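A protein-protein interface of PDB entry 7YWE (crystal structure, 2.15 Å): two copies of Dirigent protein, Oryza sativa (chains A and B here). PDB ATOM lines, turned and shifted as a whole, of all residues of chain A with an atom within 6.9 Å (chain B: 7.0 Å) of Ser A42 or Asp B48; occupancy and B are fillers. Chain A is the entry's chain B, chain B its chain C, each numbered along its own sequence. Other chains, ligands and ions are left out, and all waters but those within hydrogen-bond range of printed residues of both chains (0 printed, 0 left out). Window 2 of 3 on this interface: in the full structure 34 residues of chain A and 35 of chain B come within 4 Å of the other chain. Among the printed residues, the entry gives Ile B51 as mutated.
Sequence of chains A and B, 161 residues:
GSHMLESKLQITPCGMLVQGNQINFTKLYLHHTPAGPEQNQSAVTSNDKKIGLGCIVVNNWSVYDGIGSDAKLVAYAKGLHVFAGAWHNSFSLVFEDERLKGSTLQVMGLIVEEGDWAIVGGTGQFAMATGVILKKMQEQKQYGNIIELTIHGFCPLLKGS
NE2 of Gln A39 lies close to O of Pro A34, at 3.4 Å. O of Gln A41 is in hydrogen-bond range of NE2 of Gln A39 (2.7 Å). N of Val A58 is in hydrogen-bond range of O of Ser A42 (2.9 Å). The side-chain amide oxygen of Asn B47 lies within hydrogen-bond range of the backbone NH of Gly B54 (3.1 Å). The side-chain carboxylate (OD2) of Asp B48 lies within hydrogen-bond range of the backbone NH (N) of Ile B51. The backbone NH (N) of Asp B48 is in hydrogen-bond range of the backbone carbonyl oxygen (O) of Leu B53 (2.8 Å).
Ile B51 touches Gln A39 (CG2 to O, 3.6 Å). O of Gln A41 touches CG1 of Ile B51, at 3.9 Å. C of Gln A41 touches CD1 of Leu B53 (3.98 Å). Ser A42 touches Asp B48. Leu B53 touches Ser A42. Gly B54 touches Val A44. Val A58 touches Leu B53. Val A58 touches Gly B54. Asn A60 touches Leu B53 (CB to CD2, 3.6 Å).
Ser A42 touches just these residues of chain B: Asp B48 (3.5 Å) and Leu B53 (3.7 Å). Of the printed residues of chain A, Asp B48 touches Ser A42 (3.5 Å). Of the printed residues of chain A, Gly B54 touches Val A44 and Val A58. Of the printed residues of chain B, Val A58 touches Leu B53 and Gly B54. Of the printed residues of chain B, Asn A60 touches Leu B53. Of the printed residues of chain B, Gln A41 touches Ile B51 and Leu B53. Gly B52 touches none of the printed residues of chain A. Ala A43 touches none of the printed residues of chain B.
Printed residues of chain A that touch a printed residue of chain B: Gln A39, Gln A41, Ser A42, Val A44, Val A58 and Asn A60. Hydrophobic or aromatic side chains of chain A that line the printed part of chain B: Val A44 and Val A58. Of the 10 printed residues of chain B, 4 touch a printed residue of chain A. Among the printed residues, no Asp or Glu carboxylate lies within 4 Å of a Lys or Arg side-chain nitrogen of the other chain.
No position is printed for both chains. Of the 9 pairs that touch across the chains among the printed residues, none has its exchanged pair printed and touching as well.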
ATOM      1  N   THR A  33      20.807 -28.124 -19.343  1.00  0.00           N
ATOM      2  CA  THR A  33      21.402 -27.204 -20.312  1.00  0.00           C
ATOM      3  C   THR A  33      22.243 -26.157 -19.593  1.00  0.00           C
ATOM      4  O   THR A  33      21.752 -25.061 -19.276  1.00  0.00           O
ATOM      5  CB  THR A  33      20.316 -26.543 -21.158  1.00  0.00           C
ATOM      6  OG1 THR A  33      19.315 -27.514 -21.481  1.00  0.00           O
ATOM      7  CG2 THR A  33      20.910 -25.993 -22.447  1.00  0.00           C
ATOM      8  N   PRO A  34      23.521 -26.443 -19.325  1.00  0.00           N
ATOM      9  CA  PRO A  34      24.366 -25.475 -18.610  1.00  0.00           C
ATOM     10  C   PRO A  34      24.806 -24.273 -19.436  1.00  0.00           C
ATOM     11  O   PRO A  34      25.329 -23.312 -18.856  1.00  0.00           O
ATOM     12  CB  PRO A  34      25.586 -26.316 -18.195  1.00  0.00           C
ATOM     13  CG  PRO A  34      25.150 -27.745 -18.333  1.00  0.00           C
ATOM     14  CD  PRO A  34      24.172 -27.753 -19.458  1.00  0.00           C
ATOM     15  N   GLN A  39      19.975 -21.936 -22.025  1.00  0.00           N
ATOM     16  CA  GLN A  39      20.537 -22.257 -20.720  1.00  0.00           C
ATOM     17  C   GLN A  39      19.481 -22.109 -19.633  1.00  0.00           C
ATOM     18  O   GLN A  39      18.850 -21.056 -19.503  1.00  0.00           O
ATOM     19  CB  GLN A  39      21.731 -21.344 -20.439  1.00  0.00           C
ATOM     20  CG  GLN A  39      22.368 -21.522 -19.076  1.00  0.00           C
ATOM     21  CD  GLN A  39      23.560 -20.604 -18.882  1.00  0.00           C
ATOM     22  OE1 GLN A  39      24.081 -20.037 -19.842  1.00  0.00           O
ATOM     23  NE2 GLN A  39      23.996 -20.452 -17.638  1.00  0.00           N
ATOM     24  N   ASN A  40      19.288 -23.175 -18.847  1.00  0.00           N
ATOM     25  CA  ASN A  40      18.243 -23.216 -17.831  1.00  0.00           C
ATOM     26  C   ASN A  40      18.816 -23.394 -16.426  1.00  0.00           C
ATOM     27  O   ASN A  40      18.170 -23.979 -15.557  1.00  0.00           O
ATOM     28  CB  ASN A  40      17.227 -24.317 -18.143  1.00  0.00           C
ATOM     29  CG  ASN A  40      17.867 -25.688 -18.318  1.00  0.00           C
ATOM     30  OD1 ASN A  40      19.003 -25.923 -17.901  1.00  0.00           O
ATOM     31  ND2 ASN A  40      17.130 -26.603 -18.938  1.00  0.00           N
ATOM     32  N   GLN A  41      20.024 -22.889 -16.193  1.00  0.00           N
ATOM     33  CA  GLN A  41      20.638 -22.924 -14.872  1.00  0.00           C
ATOM     34  C   GLN A  41      21.759 -21.895 -14.845  1.00  0.00           C
ATOM     35  O   GLN A  41      22.178 -21.377 -15.883  1.00  0.00           O
ATOM     36  CB  GLN A  41      21.165 -24.322 -14.527  1.00  0.00           C
ATOM     37  CG  GLN A  41      22.404 -24.728 -15.308  1.00  0.00           C
ATOM     38  CD  GLN A  41      22.951 -26.081 -14.888  1.00  0.00           C
ATOM     39  OE1 GLN A  41      22.215 -26.936 -14.397  1.00  0.00           O
ATOM     40  NE2 GLN A  41      24.250 -26.278 -15.080  1.00  0.00           N
ATOM     41  N   SER A  42      22.244 -21.605 -13.639  1.00  0.00           N
ATOM     42  CA  SER A  42      23.305 -20.620 -13.477  1.00  0.00           C
ATOM     43  C   SER A  42      24.003 -20.841 -12.144  1.00  0.00           C
ATOM     44  O   SER A  42      23.351 -21.102 -11.131  1.00  0.00           O
ATOM     45  CB  SER A  42      22.759 -19.189 -13.551  1.00  0.00           C
ATOM     46  OG  SER A  42      23.785 -18.242 -13.303  1.00  0.00           O
ATOM     47  N   ALA A  43      25.328 -20.725 -12.156  1.00  0.00           N
ATOM     48  CA  ALA A  43      26.130 -20.836 -10.946  1.00  0.00           C
ATOM     49  C   ALA A  43      26.225 -19.476 -10.268  1.00  0.00           C
ATOM     50  O   ALA A  43      26.571 -18.477 -10.907  1.00  0.00           O
ATOM     51  CB  ALA A  43      27.528 -21.368 -11.270  1.00  0.00           C
ATOM     52  N   VAL A  44      25.915 -19.439  -8.971  1.00  0.00           N
ATOM     53  CA  VAL A  44      25.980 -18.198  -8.201  1.00  0.00           C
ATOM     54  C   VAL A  44      27.176 -18.146  -7.263  1.00  0.00           C
ATOM     55  O   VAL A  44      27.428 -17.090  -6.660  1.00  0.00           O
ATOM     56  CB  VAL A  44      24.682 -17.965  -7.401  1.00  0.00           C
ATOM     57  CG1 VAL A  44      23.517 -17.768  -8.347  1.00  0.00           C
ATOM     58  CG2 VAL A  44      24.420 -19.134  -6.459  1.00  0.00           C
ATOM     59  N   THR A  45      27.904 -19.249  -7.102  1.00  0.00           N
ATOM     60  CA  THR A  45      29.161 -19.274  -6.372  1.00  0.00           C
ATOM     61  C   THR A  45      30.177 -20.071  -7.178  1.00  0.00           C
ATOM     62  O   THR A  45      29.825 -20.815  -8.096  1.00  0.00           O
ATOM     63  CB  THR A  45      29.015 -19.893  -4.971  1.00  0.00           C
ATOM     64  OG1 THR A  45      28.627 -21.266  -5.093  1.00  0.00           O
ATOM     65  CG2 THR A  45      27.976 -19.144  -4.145  1.00  0.00           C
ATOM     66  N   ILE A  56      27.740 -23.387  -6.277  1.00  0.00           N
ATOM     67  CA  ILE A  56      26.303 -23.575  -6.127  1.00  0.00           C
ATOM     68  C   ILE A  56      25.631 -23.136  -7.419  1.00  0.00           C
ATOM     69  O   ILE A  56      25.854 -22.015  -7.892  1.00  0.00           O
ATOM     70  CB  ILE A  56      25.751 -22.787  -4.927  1.00  0.00           C
ATOM     71  CG1 ILE A  56      26.435 -23.234  -3.633  1.00  0.00           C
ATOM     72  CG2 ILE A  56      24.242 -22.948  -4.833  1.00  0.00           C
ATOM     73  CD1 ILE A  56      26.004 -22.455  -2.412  1.00  0.00           C
ATOM     74  N   VAL A  57      24.815 -24.018  -7.988  1.00  0.00           N
ATOM     75  CA  VAL A  57      24.097 -23.748  -9.227  1.00  0.00           C
ATOM     76  C   VAL A  57      22.605 -23.828  -8.941  1.00  0.00           C
ATOM     77  O   VAL A  57      22.140 -24.781  -8.303  1.00  0.00           O
ATOM     78  CB  VAL A  57      24.496 -24.734 -10.342  1.00  0.00           C
ATOM     79  CG1 VAL A  57      23.802 -24.372 -11.644  1.00  0.00           C
ATOM     80  CG2 VAL A  57      26.007 -24.753 -10.521  1.00  0.00           C
ATOM     81  N   VAL A  58      21.861 -22.825  -9.398  1.00  0.00           N
ATOM     82  CA  VAL A  58      20.406 -22.811  -9.307  1.00  0.00           C
ATOM     83  C   VAL A  58      19.846 -23.238 -10.655  1.00  0.00           C
ATOM     84  O   VAL A  58      20.191 -22.654 -11.690  1.00  0.00           O
ATOM     85  CB  VAL A  58      19.884 -21.423  -8.900  1.00  0.00           C
ATOM     86  CG1 VAL A  58      18.365 -21.408  -8.902  1.00  0.00           C
ATOM     87  CG2 VAL A  58      20.421 -21.040  -7.528  1.00  0.00           C
ATOM     88  N   ASN A  59      18.987 -24.254 -10.650  1.00  0.00           N
ATOM     89  CA  ASN A  59      18.532 -24.889 -11.878  1.00  0.00           C
ATOM     90  C   ASN A  59      17.023 -24.773 -12.034  1.00  0.00           C
ATOM     91  O   ASN A  59      16.272 -24.866 -11.058  1.00  0.00           O
ATOM     92  CB  ASN A  59      18.943 -26.368 -11.923  1.00  0.00           C
ATOM     93  CG  ASN A  59      18.679 -27.094 -10.614  1.00  0.00           C
ATOM     94  OD1 ASN A  59      19.566 -27.212  -9.771  1.00  0.00           O
ATOM     95  ND2 ASN A  59      17.460 -27.593 -10.445  1.00  0.00           N
ATOM     96  N   ASN A  60      16.593 -24.563 -13.278  1.00  0.00           N
ATOM     97  CA  ASN A  60      15.188 -24.625 -13.673  1.00  0.00           C
ATOM     98  C   ASN A  60      15.070 -25.564 -14.875  1.00  0.00           C
ATOM     99  O   ASN A  60      14.709 -25.169 -15.985  1.00  0.00           O
ATOM    100  CB  ASN A  60      14.638 -23.235 -13.986  1.00  0.00           C
ATOM    101  CG  ASN A  60      13.150 -23.246 -14.274  1.00  0.00           C
ATOM    102  OD1 ASN A  60      12.445 -24.195 -13.931  1.00  0.00           O
ATOM    103  ND2 ASN A  60      12.663 -22.187 -14.908  1.00  0.00           N
ATOM    104  N   HIS A  81      21.637 -27.354  -7.027  1.00  0.00           N
ATOM    105  CA  HIS A  81      22.563 -28.460  -6.828  1.00  0.00           C
ATOM    106  C   HIS A  81      23.946 -27.886  -6.564  1.00  0.00           C
ATOM    107  O   HIS A  81      24.380 -26.959  -7.253  1.00  0.00           O
ATOM    108  CB  HIS A  81      22.578 -29.421  -8.026  1.00  0.00           C
ATOM    109  CG  HIS A  81      22.827 -28.759  -9.346  1.00  0.00           C
ATOM    110  ND1 HIS A  81      21.942 -27.868  -9.914  1.00  0.00           N
ATOM    111  CD2 HIS A  81      23.847 -28.887 -10.228  1.00  0.00           C
ATOM    112  CE1 HIS A  81      22.414 -27.463 -11.080  1.00  0.00           C
ATOM    113  NE2 HIS A  81      23.569 -28.066 -11.293  1.00  0.00           N
ATOM    114  N   SER B  46      22.675 -12.890  -5.861  1.00  0.00           N
ATOM    115  CA  SER B  46      21.771 -12.123  -6.702  1.00  0.00           C
ATOM    116  C   SER B  46      21.244 -12.988  -7.841  1.00  0.00           C
ATOM    117  O   SER B  46      21.767 -14.067  -8.130  1.00  0.00           O
ATOM    118  CB  SER B  46      22.476 -10.885  -7.264  1.00  0.00           C
ATOM    119  OG  SER B  46      22.988 -10.072  -6.222  1.00  0.00           O
ATOM    120  N   ASN B  47      20.186 -12.502  -8.481  1.00  0.00           N
ATOM    121  CA  ASN B  47      19.677 -13.156  -9.677  1.00  0.00           C
ATOM    122  C   ASN B  47      20.594 -12.879 -10.859  1.00  0.00           C
ATOM    123  O   ASN B  47      21.068 -11.756 -11.049  1.00  0.00           O
ATOM    124  CB  ASN B  47      18.262 -12.676  -9.994  1.00  0.00           C
ATOM    125  CG  ASN B  47      17.196 -13.572  -9.405  1.00  0.00           C
ATOM    126  OD1 ASN B  47      17.432 -14.753  -9.155  1.00  0.00           O
ATOM    127  ND2 ASN B  47      16.009 -13.018  -9.187  1.00  0.00           N
ATOM    128  N   ASP B  48      20.849 -13.914 -11.655  1.00  0.00           N
ATOM    129  CA  ASP B  48      21.623 -13.754 -12.879  1.00  0.00           C
ATOM    130  C   ASP B  48      20.743 -13.102 -13.937  1.00  0.00           C
ATOM    131  O   ASP B  48      19.694 -13.645 -14.300  1.00  0.00           O
ATOM    132  CB  ASP B  48      22.150 -15.102 -13.363  1.00  0.00           C
ATOM    133  CG  ASP B  48      23.135 -14.966 -14.509  1.00  0.00           C
ATOM    134  OD1 ASP B  48      24.245 -14.440 -14.282  1.00  0.00           O
ATOM    135  OD2 ASP B  48      22.798 -15.385 -15.636  1.00  0.00           O
ATOM    136  N   LYS B  49      21.166 -11.933 -14.425  1.00  0.00           N
ATOM    137  CA  LYS B  49      20.349 -11.181 -15.372  1.00  0.00           C
ATOM    138  C   LYS B  49      20.185 -11.903 -16.703  1.00  0.00           C
ATOM    139  O   LYS B  49      19.199 -11.661 -17.408  1.00  0.00           O
ATOM    140  CB  LYS B  49      20.958  -9.796 -15.601  1.00  0.00           C
ATOM    141  CG  LYS B  49      22.391  -9.824 -16.111  1.00  0.00           C
ATOM    142  N   LYS B  50      21.119 -12.785 -17.062  1.00  0.00           N
ATOM    143  CA  LYS B  50      21.040 -13.464 -18.349  1.00  0.00           C
ATOM    144  C   LYS B  50      19.985 -14.565 -18.347  1.00  0.00           C
ATOM    145  O   LYS B  50      19.251 -14.724 -19.330  1.00  0.00           O
ATOM    146  CB  LYS B  50      22.407 -14.039 -18.722  1.00  0.00           C
ATOM    147  N   ILE B  51      19.890 -15.326 -17.262  1.00  0.00           N
ATOM    148  CA  ILE B  51      18.993 -16.472 -17.193  1.00  0.00           C
ATOM    149  C   ILE B  51      17.709 -16.141 -16.441  1.00  0.00           C
ATOM    150  O   ILE B  51      16.636 -16.623 -16.802  1.00  0.00           O
ATOM    151  CB  ILE B  51      19.718 -17.676 -16.554  1.00  0.00           C
ATOM    152  CG1 ILE B  51      21.066 -17.909 -17.239  1.00  0.00           C
ATOM    153  CG2 ILE B  51      18.861 -18.930 -16.643  1.00  0.00           C
ATOM    154  CD1 ILE B  51      20.959 -18.141 -18.731  1.00  0.00           C
ATOM    155  N   GLY B  52      17.800 -15.323 -15.401  1.00  0.00           N
ATOM    156  CA  GLY B  52      16.649 -14.960 -14.609  1.00  0.00           C
ATOM    157  C   GLY B  52      16.457 -15.763 -13.344  1.00  0.00           C
ATOM    158  O   GLY B  52      15.317 -15.893 -12.881  1.00  0.00           O
ATOM    159  N   LEU B  53      17.526 -16.308 -12.772  1.00  0.00           N
ATOM    160  CA  LEU B  53      17.430 -17.120 -11.570  1.00  0.00           C
ATOM    161  C   LEU B  53      18.752 -17.038 -10.823  1.00  0.00           C
ATOM    162  O   LEU B  53      19.742 -16.503 -11.327  1.00  0.00           O
ATOM    163  CB  LEU B  53      17.061 -18.572 -11.908  1.00  0.00           C
ATOM    164  CG  LEU B  53      17.733 -19.254 -13.107  1.00  0.00           C
ATOM    165  CD1 LEU B  53      19.162 -19.683 -12.801  1.00  0.00           C
ATOM    166  CD2 LEU B  53      16.910 -20.444 -13.574  1.00  0.00           C
ATOM    167  N   GLY B  54      18.756 -17.565  -9.603  1.00  0.00           N
ATOM    168  CA  GLY B  54      19.967 -17.666  -8.810  1.00  0.00           C
ATOM    169  C   GLY B  54      19.928 -16.959  -7.474  1.00  0.00           C
ATOM    170  O   GLY B  54      20.856 -17.142  -6.672  1.00  0.00           O
ATOM    171  N   CYS B  55      18.905 -16.159  -7.188  1.00  0.00           N
ATOM    172  CA  CYS B  55      18.838 -15.474  -5.905  1.00  0.00           C
ATOM    173  C   CYS B  55      18.626 -16.479  -4.780  1.00  0.00           C
ATOM    174  O   CYS B  55      17.692 -17.286  -4.820  1.00  0.00           O
ATOM    175  CB  CYS B  55      17.714 -14.439  -5.908  1.00  0.00           C
ATOM    176  SG  CYS B  55      17.601 -13.484  -4.379  1.00  0.00           S
